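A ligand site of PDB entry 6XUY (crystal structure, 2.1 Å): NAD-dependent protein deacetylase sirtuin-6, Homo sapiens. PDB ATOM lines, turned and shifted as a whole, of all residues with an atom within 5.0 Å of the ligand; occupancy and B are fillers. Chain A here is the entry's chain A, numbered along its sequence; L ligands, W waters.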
ATOM      1  N   GLU A  16      28.262  16.151  29.819  1.00  0.00           N
ATOM      2  CA  GLU A  16      29.107  15.298  28.978  1.00  0.00           C
ATOM      3  C   GLU A  16      30.287  14.733  29.788  1.00  0.00           C
ATOM      4  O   GLU A  16      30.736  15.336  30.734  1.00  0.00           O
ATOM      5  CB  GLU A  16      29.454  16.038  27.716  1.00  0.00           C
ATOM      6  CG  GLU A  16      28.219  16.219  26.856  1.00  0.00           C
ATOM      7  CD  GLU A  16      28.495  16.969  25.600  1.00  0.00           C
ATOM      8  OE1 GLU A  16      29.454  17.747  25.663  1.00  0.00           O
ATOM      9  OE2 GLU A  16      27.719  16.867  24.597  1.00  0.00           O
ATOM     10  N   GLY A  46      20.658   6.347  17.999  1.00  0.00           N
ATOM     11  CA  GLY A  46      19.806   7.463  18.357  1.00  0.00           C
ATOM     12  C   GLY A  46      20.438   8.760  17.915  1.00  0.00           C
ATOM     13  O   GLY A  46      21.473   8.669  17.208  1.00  0.00           O
ATOM     14  N   ALA A  47      19.840   9.871  18.369  1.00  0.00           N
ATOM     15  CA  ALA A  47      19.965  11.175  17.695  1.00  0.00           C
ATOM     16  C   ALA A  47      21.391  11.674  17.695  1.00  0.00           C
ATOM     17  O   ALA A  47      21.714  12.378  16.806  1.00  0.00           O
ATOM     18  CB  ALA A  47      19.025  12.199  18.290  1.00  0.00           C
ATOM     19  N   GLY A  48      22.226  11.260  18.645  1.00  0.00           N
ATOM     20  CA  GLY A  48      23.648  11.644  18.745  1.00  0.00           C
ATOM     21  C   GLY A  48      24.494  11.137  17.567  1.00  0.00           C
ATOM     22  O   GLY A  48      25.501  11.712  17.320  1.00  0.00           O
ATOM     23  N   THR A  51      24.274  14.446  15.037  1.00  0.00           N
ATOM     24  CA  THR A  51      24.637  15.811  15.447  1.00  0.00           C
ATOM     25  C   THR A  51      25.740  16.366  14.523  1.00  0.00           C
ATOM     26  O   THR A  51      25.725  17.526  14.289  1.00  0.00           O
ATOM     27  CB  THR A  51      24.954  15.805  16.961  1.00  0.00           C
ATOM     28  OG1 THR A  51      25.788  14.711  17.332  1.00  0.00           O
ATOM     29  CG2 THR A  51      23.692  15.800  17.767  1.00  0.00           C
ATOM     30  N   ASP A  57      20.238  16.782  18.773  1.00  0.00           N
ATOM     31  CA  ASP A  57      19.610  15.636  19.469  1.00  0.00           C
ATOM     32  C   ASP A  57      18.417  16.195  20.272  1.00  0.00           C
ATOM     33  O   ASP A  57      17.979  17.362  20.076  1.00  0.00           O
ATOM     34  CB  ASP A  57      20.676  14.864  20.267  1.00  0.00           C
ATOM     35  CG  ASP A  57      21.461  15.676  21.292  1.00  0.00           C
ATOM     36  OD1 ASP A  57      21.087  16.782  21.587  1.00  0.00           O
ATOM     37  OD2 ASP A  57      22.428  15.160  21.836  1.00  0.00           O
ATOM     38  N   PHE A  58      17.895  15.390  21.198  1.00  0.00           N
ATOM     39  CA  PHE A  58      16.769  15.760  22.078  1.00  0.00           C
ATOM     40  C   PHE A  58      17.313  16.269  23.417  1.00  0.00           C
ATOM     41  O   PHE A  58      16.758  17.204  23.916  1.00  0.00           O
ATOM     42  CB  PHE A  58      15.851  14.529  22.186  1.00  0.00           C
ATOM     43  CG  PHE A  58      15.181  14.245  20.883  1.00  0.00           C
ATOM     44  CD1 PHE A  58      14.033  14.909  20.542  1.00  0.00           C
ATOM     45  CD2 PHE A  58      15.734  13.358  19.980  1.00  0.00           C
ATOM     46  CE1 PHE A  58      13.429  14.663  19.326  1.00  0.00           C
ATOM     47  CE2 PHE A  58      15.110  13.107  18.778  1.00  0.00           C
ATOM     48  CZ  PHE A  58      13.981  13.806  18.427  1.00  0.00           C
ATOM     49  N   ARG A  59      18.279  15.589  24.009  1.00  0.00           N
ATOM     50  CA  ARG A  59      18.603  15.658  25.432  1.00  0.00           C
ATOM     51  C   ARG A  59      20.084  15.957  25.690  1.00  0.00           C
ATOM     52  O   ARG A  59      20.395  16.066  26.909  1.00  0.00           O
ATOM     53  CB  ARG A  59      18.159  14.395  26.196  1.00  0.00           C
ATOM     54  CG  ARG A  59      16.720  14.014  25.849  1.00  0.00           C
ATOM     55  CD  ARG A  59      16.271  12.904  26.847  1.00  0.00           C
ATOM     56  NE  ARG A  59      14.891  12.578  26.532  1.00  0.00           N
ATOM     57  CZ  ARG A  59      14.455  11.928  25.441  1.00  0.00           C
ATOM     58  NH1 ARG A  59      15.279  11.540  24.475  1.00  0.00           N
ATOM     59  NH2 ARG A  59      13.155  11.679  25.285  1.00  0.00           N
ATOM     60  N   GLY A  60      20.869  16.277  24.659  1.00  0.00           N
ATOM     61  CA  GLY A  60      22.256  16.818  24.759  1.00  0.00           C
ATOM     62  C   GLY A  60      22.248  18.267  25.243  1.00  0.00           C
ATOM     63  O   GLY A  60      21.166  18.875  25.413  1.00  0.00           O
ATOM     64  N   TRP A  65      14.595  19.094  23.400  1.00  0.00           N
ATOM     65  CA  TRP A  65      13.969  19.107  24.739  1.00  0.00           C
ATOM     66  C   TRP A  65      14.815  19.926  25.745  1.00  0.00           C
ATOM     67  O   TRP A  65      14.251  20.638  26.554  1.00  0.00           O
ATOM     68  CB  TRP A  65      13.762  17.695  25.282  1.00  0.00           C
ATOM     69  CG  TRP A  65      12.985  16.728  24.437  1.00  0.00           C
ATOM     70  CD1 TRP A  65      13.041  15.360  24.537  1.00  0.00           C
ATOM     71  CD2 TRP A  65      11.993  17.003  23.434  1.00  0.00           C
ATOM     72  NE1 TRP A  65      12.158  14.770  23.658  1.00  0.00           N
ATOM     73  CE2 TRP A  65      11.510  15.756  22.970  1.00  0.00           C
ATOM     74  CE3 TRP A  65      11.398  18.176  22.955  1.00  0.00           C
ATOM     75  CZ2 TRP A  65      10.523  15.675  21.997  1.00  0.00           C
ATOM     76  CZ3 TRP A  65      10.509  18.093  21.909  1.00  0.00           C
ATOM     77  CH2 TRP A  65      10.050  16.844  21.463  1.00  0.00           C
ATOM     78  N   GLN A 107      16.143   4.721  16.638  1.00  0.00           N
ATOM     79  CA  GLN A 107      15.050   5.529  17.125  1.00  0.00           C
ATOM     80  C   GLN A 107      14.947   6.768  16.264  1.00  0.00           C
ATOM     81  O   GLN A 107      14.083   7.562  16.584  1.00  0.00           O
ATOM     82  CB  GLN A 107      15.345   5.842  18.578  1.00  0.00           C
ATOM     83  CG  GLN A 107      15.479   4.588  19.398  1.00  0.00           C
ATOM     84  CD  GLN A 107      15.734   4.869  20.852  1.00  0.00           C
ATOM     85  OE1 GLN A 107      14.887   5.430  21.523  1.00  0.00           O
ATOM     86  NE2 GLN A 107      16.901   4.500  21.340  1.00  0.00           N
ATOM     87  N   ASN A 108      15.870   6.965  15.319  1.00  0.00           N
ATOM     88  CA  ASN A 108      15.927   8.261  14.561  1.00  0.00           C
ATOM     89  C   ASN A 108      14.867   8.254  13.487  1.00  0.00           C
ATOM     90  O   ASN A 108      14.705   7.203  12.858  1.00  0.00           O
ATOM     91  CB  ASN A 108      17.263   8.513  13.865  1.00  0.00           C
ATOM     92  CG  ASN A 108      18.413   8.490  14.843  1.00  0.00           C
ATOM     93  OD1 ASN A 108      18.163   8.654  15.991  1.00  0.00           O
ATOM     94  ND2 ASN A 108      19.648   8.317  14.391  1.00  0.00           N
ATOM     95  N   HIS A 127      10.732   4.770  15.522  1.00  0.00           N
ATOM     96  CA  HIS A 127       9.937   5.997  15.745  1.00  0.00           C
ATOM     97  C   HIS A 127       9.475   6.521  14.387  1.00  0.00           C
ATOM     98  O   HIS A 127       8.959   7.676  14.357  1.00  0.00           O
ATOM     99  CB  HIS A 127      10.742   6.996  16.590  1.00  0.00           C
ATOM    100  CG  HIS A 127      11.096   6.454  17.934  1.00  0.00           C
ATOM    101  ND1 HIS A 127      12.027   7.047  18.744  1.00  0.00           N
ATOM    102  CD2 HIS A 127      10.658   5.335  18.560  1.00  0.00           C
ATOM    103  CE1 HIS A 127      12.126   6.371  19.827  1.00  0.00           C
ATOM    104  NE2 HIS A 127      11.269   5.281  19.731  1.00  0.00           N
ATOM    105  N   TRP A 182       3.303  11.017  20.784  1.00  0.00           N
ATOM    106  CA  TRP A 182       3.552  10.509  22.152  1.00  0.00           C
ATOM    107  C   TRP A 182       2.655   9.304  22.438  1.00  0.00           C
ATOM    108  O   TRP A 182       3.156   8.335  22.984  1.00  0.00           O
ATOM    109  CB  TRP A 182       3.377  11.628  23.195  1.00  0.00           C
ATOM    110  CG  TRP A 182       4.388  12.716  23.037  1.00  0.00           C
ATOM    111  CD1 TRP A 182       4.231  13.896  22.351  1.00  0.00           C
ATOM    112  CD2 TRP A 182       5.757  12.693  23.484  1.00  0.00           C
ATOM    113  NE1 TRP A 182       5.394  14.630  22.380  1.00  0.00           N
ATOM    114  CE2 TRP A 182       6.346  13.914  23.075  1.00  0.00           C
ATOM    115  CE3 TRP A 182       6.531  11.797  24.241  1.00  0.00           C
ATOM    116  CZ2 TRP A 182       7.670  14.238  23.396  1.00  0.00           C
ATOM    117  CZ3 TRP A 182       7.844  12.104  24.526  1.00  0.00           C
ATOM    118  CH2 TRP A 182       8.404  13.322  24.110  1.00  0.00           C
ATOM    119  N   GLY A 208      25.140   7.081  20.518  1.00  0.00           N
ATOM    120  CA  GLY A 208      24.410   8.394  20.548  1.00  0.00           C
ATOM    121  C   GLY A 208      22.902   8.211  20.856  1.00  0.00           C
ATOM    122  O   GLY A 208      22.031   8.888  20.222  1.00  0.00           O
ATOM    123  N   THR A 209      22.567   7.365  21.831  1.00  0.00           N
ATOM    124  CA  THR A 209      21.213   7.251  22.435  1.00  0.00           C
ATOM    125  C   THR A 209      21.313   7.245  23.984  1.00  0.00           C
ATOM    126  O   THR A 209      22.239   6.652  24.520  1.00  0.00           O
ATOM    127  CB  THR A 209      20.456   6.033  21.893  1.00  0.00           C
ATOM    128  OG1 THR A 209      19.239   5.999  22.649  1.00  0.00           O
ATOM    129  CG2 THR A 209      21.135   4.699  22.080  1.00  0.00           C
ATOM    130  N   SER A 210      20.401   7.931  24.685  1.00  0.00           N
ATOM    131  CA  SER A 210      20.427   8.045  26.142  1.00  0.00           C
ATOM    132  C   SER A 210      19.575   6.939  26.762  1.00  0.00           C
ATOM    133  O   SER A 210      19.736   6.744  27.996  1.00  0.00           O
ATOM    134  CB  SER A 210      20.068   9.448  26.657  1.00  0.00           C
ATOM    135  OG  SER A 210      18.768   9.842  26.261  1.00  0.00           O
ATOM    136  N   LEU A 211      18.937   6.117  25.939  1.00  0.00           N
ATOM    137  CA  LEU A 211      18.226   4.862  26.329  1.00  0.00           C
ATOM    138  C   LEU A 211      17.097   5.101  27.312  1.00  0.00           C
ATOM    139  O   LEU A 211      16.785   4.213  28.057  1.00  0.00           O
ATOM    140  CB  LEU A 211      19.290   3.895  26.873  1.00  0.00           C
ATOM    141  CG  LEU A 211      20.326   3.482  25.827  1.00  0.00           C
ATOM    142  CD1 LEU A 211      21.436   2.650  26.438  1.00  0.00           C
ATOM    143  CD2 LEU A 211      19.684   2.717  24.703  1.00  0.00           C
ATOM    144  N   GLN A 212      16.446   6.251  27.236  1.00  0.00           N
ATOM    145  CA  GLN A 212      15.471   6.701  28.267  1.00  0.00           C
ATOM    146  C   GLN A 212      14.049   6.331  27.833  1.00  0.00           C
ATOM    147  O   GLN A 212      13.150   6.541  28.641  1.00  0.00           O
ATOM    148  CB  GLN A 212      15.589   8.205  28.466  1.00  0.00           C
ATOM    149  CG  GLN A 212      16.922   8.643  29.070  1.00  0.00           C
ATOM    150  CD  GLN A 212      16.893  10.090  29.454  1.00  0.00           C
ATOM    151  OE1 GLN A 212      16.015  10.502  30.214  1.00  0.00           O
ATOM    152  NE2 GLN A 212      17.857  10.882  28.986  1.00  0.00           N
ATOM    153  N   ILE A 213      13.842   6.001  26.570  1.00  0.00           N
ATOM    154  CA  ILE A 213      12.542   5.661  25.971  1.00  0.00           C
ATOM    155  C   ILE A 213      12.279   4.177  26.103  1.00  0.00           C
ATOM    156  O   ILE A 213      13.146   3.387  25.638  1.00  0.00           O
ATOM    157  CB  ILE A 213      12.489   6.093  24.494  1.00  0.00           C
ATOM    158  CG1 ILE A 213      12.500   7.609  24.352  1.00  0.00           C
ATOM    159  CG2 ILE A 213      11.287   5.460  23.786  1.00  0.00           C
ATOM    160  CD1 ILE A 213      11.221   8.267  24.843  1.00  0.00           C
ATOM    161  N   ASN A 234      28.404   7.044  24.044  1.00  0.00           N
ATOM    162  CA  ASN A 234      27.552   8.176  24.409  1.00  0.00           C
ATOM    163  C   ASN A 234      28.378   9.220  25.159  1.00  0.00           C
ATOM    164  O   ASN A 234      29.125   8.851  26.046  1.00  0.00           O
ATOM    165  CB  ASN A 234      26.331   7.780  25.238  1.00  0.00           C
ATOM    166  CG  ASN A 234      25.168   8.685  24.906  1.00  0.00           C
ATOM    167  OD1 ASN A 234      24.792   8.796  23.757  1.00  0.00           O
ATOM    168  ND2 ASN A 234      24.573   9.353  25.915  1.00  0.00           N
ATOM    169  N   LEU A 235      28.209  10.494  24.804  1.00  0.00           N
ATOM    170  CA  LEU A 235      28.916  11.594  25.483  1.00  0.00           C
ATOM    171  C   LEU A 235      28.318  11.827  26.891  1.00  0.00           C
ATOM    172  O   LEU A 235      29.110  12.165  27.807  1.00  0.00           O
ATOM    173  CB  LEU A 235      28.829  12.868  24.643  1.00  0.00           C
ATOM    174  CG  LEU A 235      29.841  12.920  23.504  1.00  0.00           C
ATOM    175  CD1 LEU A 235      29.505  14.070  22.577  1.00  0.00           C
ATOM    176  CD2 LEU A 235      31.226  13.102  24.150  1.00  0.00           C
ATOM    177  N   GLN A 236      27.021  11.581  27.044  1.00  0.00           N
ATOM    178  CA  GLN A 236      26.313  11.708  28.335  1.00  0.00           C
ATOM    179  C   GLN A 236      26.090  10.330  28.935  1.00  0.00           C
ATOM    180  O   GLN A 236      26.172   9.295  28.264  1.00  0.00           O
ATOM    181  CB  GLN A 236      24.928  12.325  28.249  1.00  0.00           C
ATOM    182  CG  GLN A 236      24.897  13.807  27.934  1.00  0.00           C
ATOM    183  CD  GLN A 236      23.510  14.323  27.623  1.00  0.00           C
ATOM    184  OE1 GLN A 236      22.644  13.581  27.170  1.00  0.00           O
ATOM    185  NE2 GLN A 236      23.242  15.594  27.909  1.00  0.00           N
ATOM    186  N   PRO A 237      25.834  10.305  30.250  1.00  0.00           N
ATOM    187  CA  PRO A 237      25.281   9.135  30.911  1.00  0.00           C
ATOM    188  C   PRO A 237      24.017   8.686  30.168  1.00  0.00           C
ATOM    189  O   PRO A 237      23.268   9.466  29.631  1.00  0.00           O
ATOM    190  CB  PRO A 237      24.938   9.599  32.331  1.00  0.00           C
ATOM    191  CG  PRO A 237      25.848  10.791  32.542  1.00  0.00           C
ATOM    192  CD  PRO A 237      25.943  11.462  31.180  1.00  0.00           C
ATOM    193  N   GLY A 250      32.847   9.423  24.168  1.00  0.00           N
ATOM    194  CA  GLY A 250      33.452  10.151  23.033  1.00  0.00           C
ATOM    195  C   GLY A 250      32.494  10.312  21.867  1.00  0.00           C
ATOM    196  O   GLY A 250      31.373   9.738  21.890  1.00  0.00           O
ATOM    197  N   TYR A 251      32.885  11.166  20.945  1.00  0.00           N
ATOM    198  CA  TYR A 251      32.236  11.345  19.627  1.00  0.00           C
ATOM    199  C   TYR A 251      32.187  10.018  18.894  1.00  0.00           C
ATOM    200  O   TYR A 251      33.199   9.381  18.779  1.00  0.00           O
ATOM    201  CB  TYR A 251      33.065  12.376  18.841  1.00  0.00           C
ATOM    202  CG  TYR A 251      33.032  13.710  19.499  1.00  0.00           C
ATOM    203  CD1 TYR A 251      31.837  14.392  19.583  1.00  0.00           C
ATOM    204  CD2 TYR A 251      34.109  14.204  20.243  1.00  0.00           C
ATOM    205  CE1 TYR A 251      31.743  15.583  20.271  1.00  0.00           C
ATOM    206  CE2 TYR A 251      34.021  15.425  20.872  1.00  0.00           C
ATOM    207  CZ  TYR A 251      32.855  16.157  20.807  1.00  0.00           C
ATOM    208  OH  TYR A 251      32.640  17.331  21.491  1.00  0.00           O
ATOM    209  N   VAL A 252      31.009   9.647  18.412  1.00  0.00           N
ATOM    210  CA  VAL A 252      30.820   8.360  17.706  1.00  0.00           C
ATOM    211  C   VAL A 252      31.675   8.326  16.429  1.00  0.00           C
ATOM    212  O   VAL A 252      32.279   7.334  16.185  1.00  0.00           O
ATOM    213  CB  VAL A 252      29.353   8.104  17.406  1.00  0.00           C
ATOM    214  CG1 VAL A 252      28.705   7.661  18.697  1.00  0.00           C
ATOM    215  CG2 VAL A 252      28.655   9.361  16.816  1.00  0.00           C
HETATM  216  N1  LIG L   1      28.891  11.527  19.741  1.00  0.00           N
HETATM  217  C1  LIG L   1      28.516  10.832  20.851  1.00  0.00           C
HETATM  218  N2  LIG L   1      27.435  11.014  21.625  1.00  0.00           N
HETATM  219  C2  LIG L   1      26.671  12.027  21.160  1.00  0.00           C
HETATM  220  C3  LIG L   1      26.959  12.856  20.091  1.00  0.00           C
HETATM  221  C4  LIG L   1      28.140  12.592  19.345  1.00  0.00           C
HETATM  222  N3  LIG L   1      28.537  13.284  18.243  1.00  0.00           N
HETATM  223  N4  LIG L   1      25.928  13.791  19.922  1.00  0.00           N
HETATM  224  C5  LIG L   1      25.048  13.551  20.852  1.00  0.00           C
HETATM  225  N5  LIG L   1      25.450  12.446  21.638  1.00  0.00           N
HETATM  226  P1  LIG L   1      18.766  11.726  22.929  1.00  0.00           P
HETATM  227  P2  LIG L   1      17.504   9.413  21.735  1.00  0.00           P
HETATM  228  C6  LIG L   1      24.673  11.914  22.726  1.00  0.00           C
HETATM  229  O1  LIG L   1      17.914  11.499  24.142  1.00  0.00           O
HETATM  230  O2  LIG L   1      17.824   8.911  20.348  1.00  0.00           O
HETATM  231  C7  LIG L   1      12.864  11.392  21.750  1.00  0.00           C
HETATM  232  O3  LIG L   1      11.689  11.868  22.271  1.00  0.00           O
HETATM  233  C8  LIG L   1      24.015  12.938  23.630  1.00  0.00           C
HETATM  234  O4  LIG L   1      24.850  13.014  24.755  1.00  0.00           O
HETATM  235  O5  LIG L   1      19.104  13.148  22.523  1.00  0.00           O
HETATM  236  O6  LIG L   1      18.284   8.646  22.812  1.00  0.00           O
HETATM  237  C9  LIG L   1      12.722  10.964  20.285  1.00  0.00           C
HETATM  238  O7  LIG L   1      11.529  10.272  20.095  1.00  0.00           O
HETATM  239  C10 LIG L   1      22.727  12.234  24.104  1.00  0.00           C
HETATM  240  O8  LIG L   1      22.898  11.482  25.278  1.00  0.00           O
HETATM  241  O9  LIG L   1      18.168  10.906  21.678  1.00  0.00           O
HETATM  242  C11 LIG L   1      13.868   9.973  20.103  1.00  0.00           C
HETATM  243  O10 LIG L   1      13.617   9.065  19.029  1.00  0.00           O
HETATM  244  C12 LIG L   1      22.512  11.129  23.081  1.00  0.00           C
HETATM  245  O11 LIG L   1      23.589  11.261  22.153  1.00  0.00           O
HETATM  246  C13 LIG L   1      13.796   9.251  21.453  1.00  0.00           C
HETATM  247  O12 LIG L   1      13.249  10.167  22.421  1.00  0.00           O
HETATM  248  C14 LIG L   1      21.245  11.264  22.286  1.00  0.00           C
HETATM  249  O13 LIG L   1      20.093  10.891  23.164  1.00  0.00           O
HETATM  250  C15 LIG L   1      15.053   8.673  22.020  1.00  0.00           C
HETATM  251  O14 LIG L   1      15.994   9.707  21.964  1.00  0.00           O
HETATM  252  O   HOH W   1      27.251  12.816  15.421  1.00  0.00           O
HETATM  253  O   HOH W   2      30.254  11.892  16.033  1.00  0.00           O
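O of Gly 48 sits close to N4 of the ligand (3.4 Å). The backbone carbonyl oxygen (O) of Gly 208 sits close to an oxygen (O11) of the ligand, at 3.4 Å. Merely in contact with the ligand: Gly 46, Asp 57, Ile 213, Gly 250 and Tyr 251. Hydrophobic or aromatic side chains that line the ligand: Ala 47, Phe 58, Trp 65, His 127, Ile 213, Leu 235, Tyr 251 and Val 252. Of the 27 residues printed, 20 come within 4 Å of the ligand. The nearest printed residue that does not touch the ligand is Trp 182 (4.04 Å).
Water W2 bridges a nitrogen (N3) of the ligand (3.1 Å) and the backbone NH of Val 252 (3.4 Å). Water W1 lies within hydrogen-bond range of the backbone carbonyl oxygen (O) of Gly 48, the side-chain hydroxyl (OG1) of Thr 51 and a nitrogen (N3) of the ligand.
The side-chain hydroxyl (OG1) of Thr 51 is in hydrogen-bond range of the backbone carbonyl oxygen (O) of Gly 48 (3.0 Å). The side-chain hydroxyl (OG1) of Thr 209 sits at hydrogen-bond distance from the side-chain amide nitrogen (NE2) of Gln 107. The side-chain hydroxyl (OG1) of Thr 209 sits close to the backbone NH (N) of Leu 211 (3.3 Å). The backbone NH (N) of Trp 65 sits at hydrogen-bond distance from the backbone carbonyl oxygen (O) of Phe 58 (2.9 Å). The backbone NH (N) of Ala 47 lies within hydrogen-bond range of the side-chain amide oxygen (OD1) of Asn 108, 3.2 Å away. O of Gly 46 lies within hydrogen-bond range of ND2 of Asn 108, 3.4 Å away. The backbone carbonyl oxygen (O) of Gly 208 lies within hydrogen-bond range of the backbone NH (N) of Gly 48 (2.9 Å). N of Gly 60 lies within hydrogen-bond range of OD1 of Asp 57 (3.1 Å).
A ring nitrogen (ND1) of His 127 is in hydrogen-bond range of an oxygen (O10) of the ligand, 2.6 Å away. O5 of the ligand is in hydrogen-bond range of N of Arg 59. An oxygen (O1) of the ligand lies within salt-bridge range of the guanidinium group (NH1) of Arg 59. A nitrogen (N4) of the ligand lies within hydrogen-bond range of the side-chain hydroxyl of Thr 51 (2.8 Å). The side-chain amide nitrogen of Asn 234 sits at hydrogen-bond distance from an oxygen (O8) of the ligand, 2.8 Å away. The side-chain hydroxyl (OG1) of Thr 209 is in hydrogen-bond range of an oxygen (O6) of the ligand, 2.8 Å away. N of Ser 210 sits at hydrogen-bond distance from O6 of the ligand, at 2.9 Å. The side-chain hydroxyl (OG) of Ser 210 is in hydrogen-bond range of an oxygen (O1) of the ligand. The backbone NH (N) of Gln 236 lies close to an oxygen (O4) of the ligand. The side-chain amide oxygen of Gln 236 sits at hydrogen-bond distance from an oxygen (O8) of the ligand. The backbone NH of Phe 58 sits at hydrogen-bond distance from an oxygen (O5) of the ligand (2.9 Å). An oxygen (O10) of the ligand is in hydrogen-bond range of the backbone carbonyl oxygen of Gln 107, at 2.9 Å. An oxygen (O2) of the ligand sits at hydrogen-bond distance from the backbone NH of Ala 47 (3.0 Å). The backbone NH (N) of Val 252 lies within hydrogen-bond range of a nitrogen (N1) of the ligand. An oxygen (O3) of the ligand is in hydrogen-bond range of the indole nitrogen of Trp 65 (3.3 Å). A nitrogen (N2) of the ligand lies within hydrogen-bond range of the backbone NH (N) of Leu 235, at 3.3 Å.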
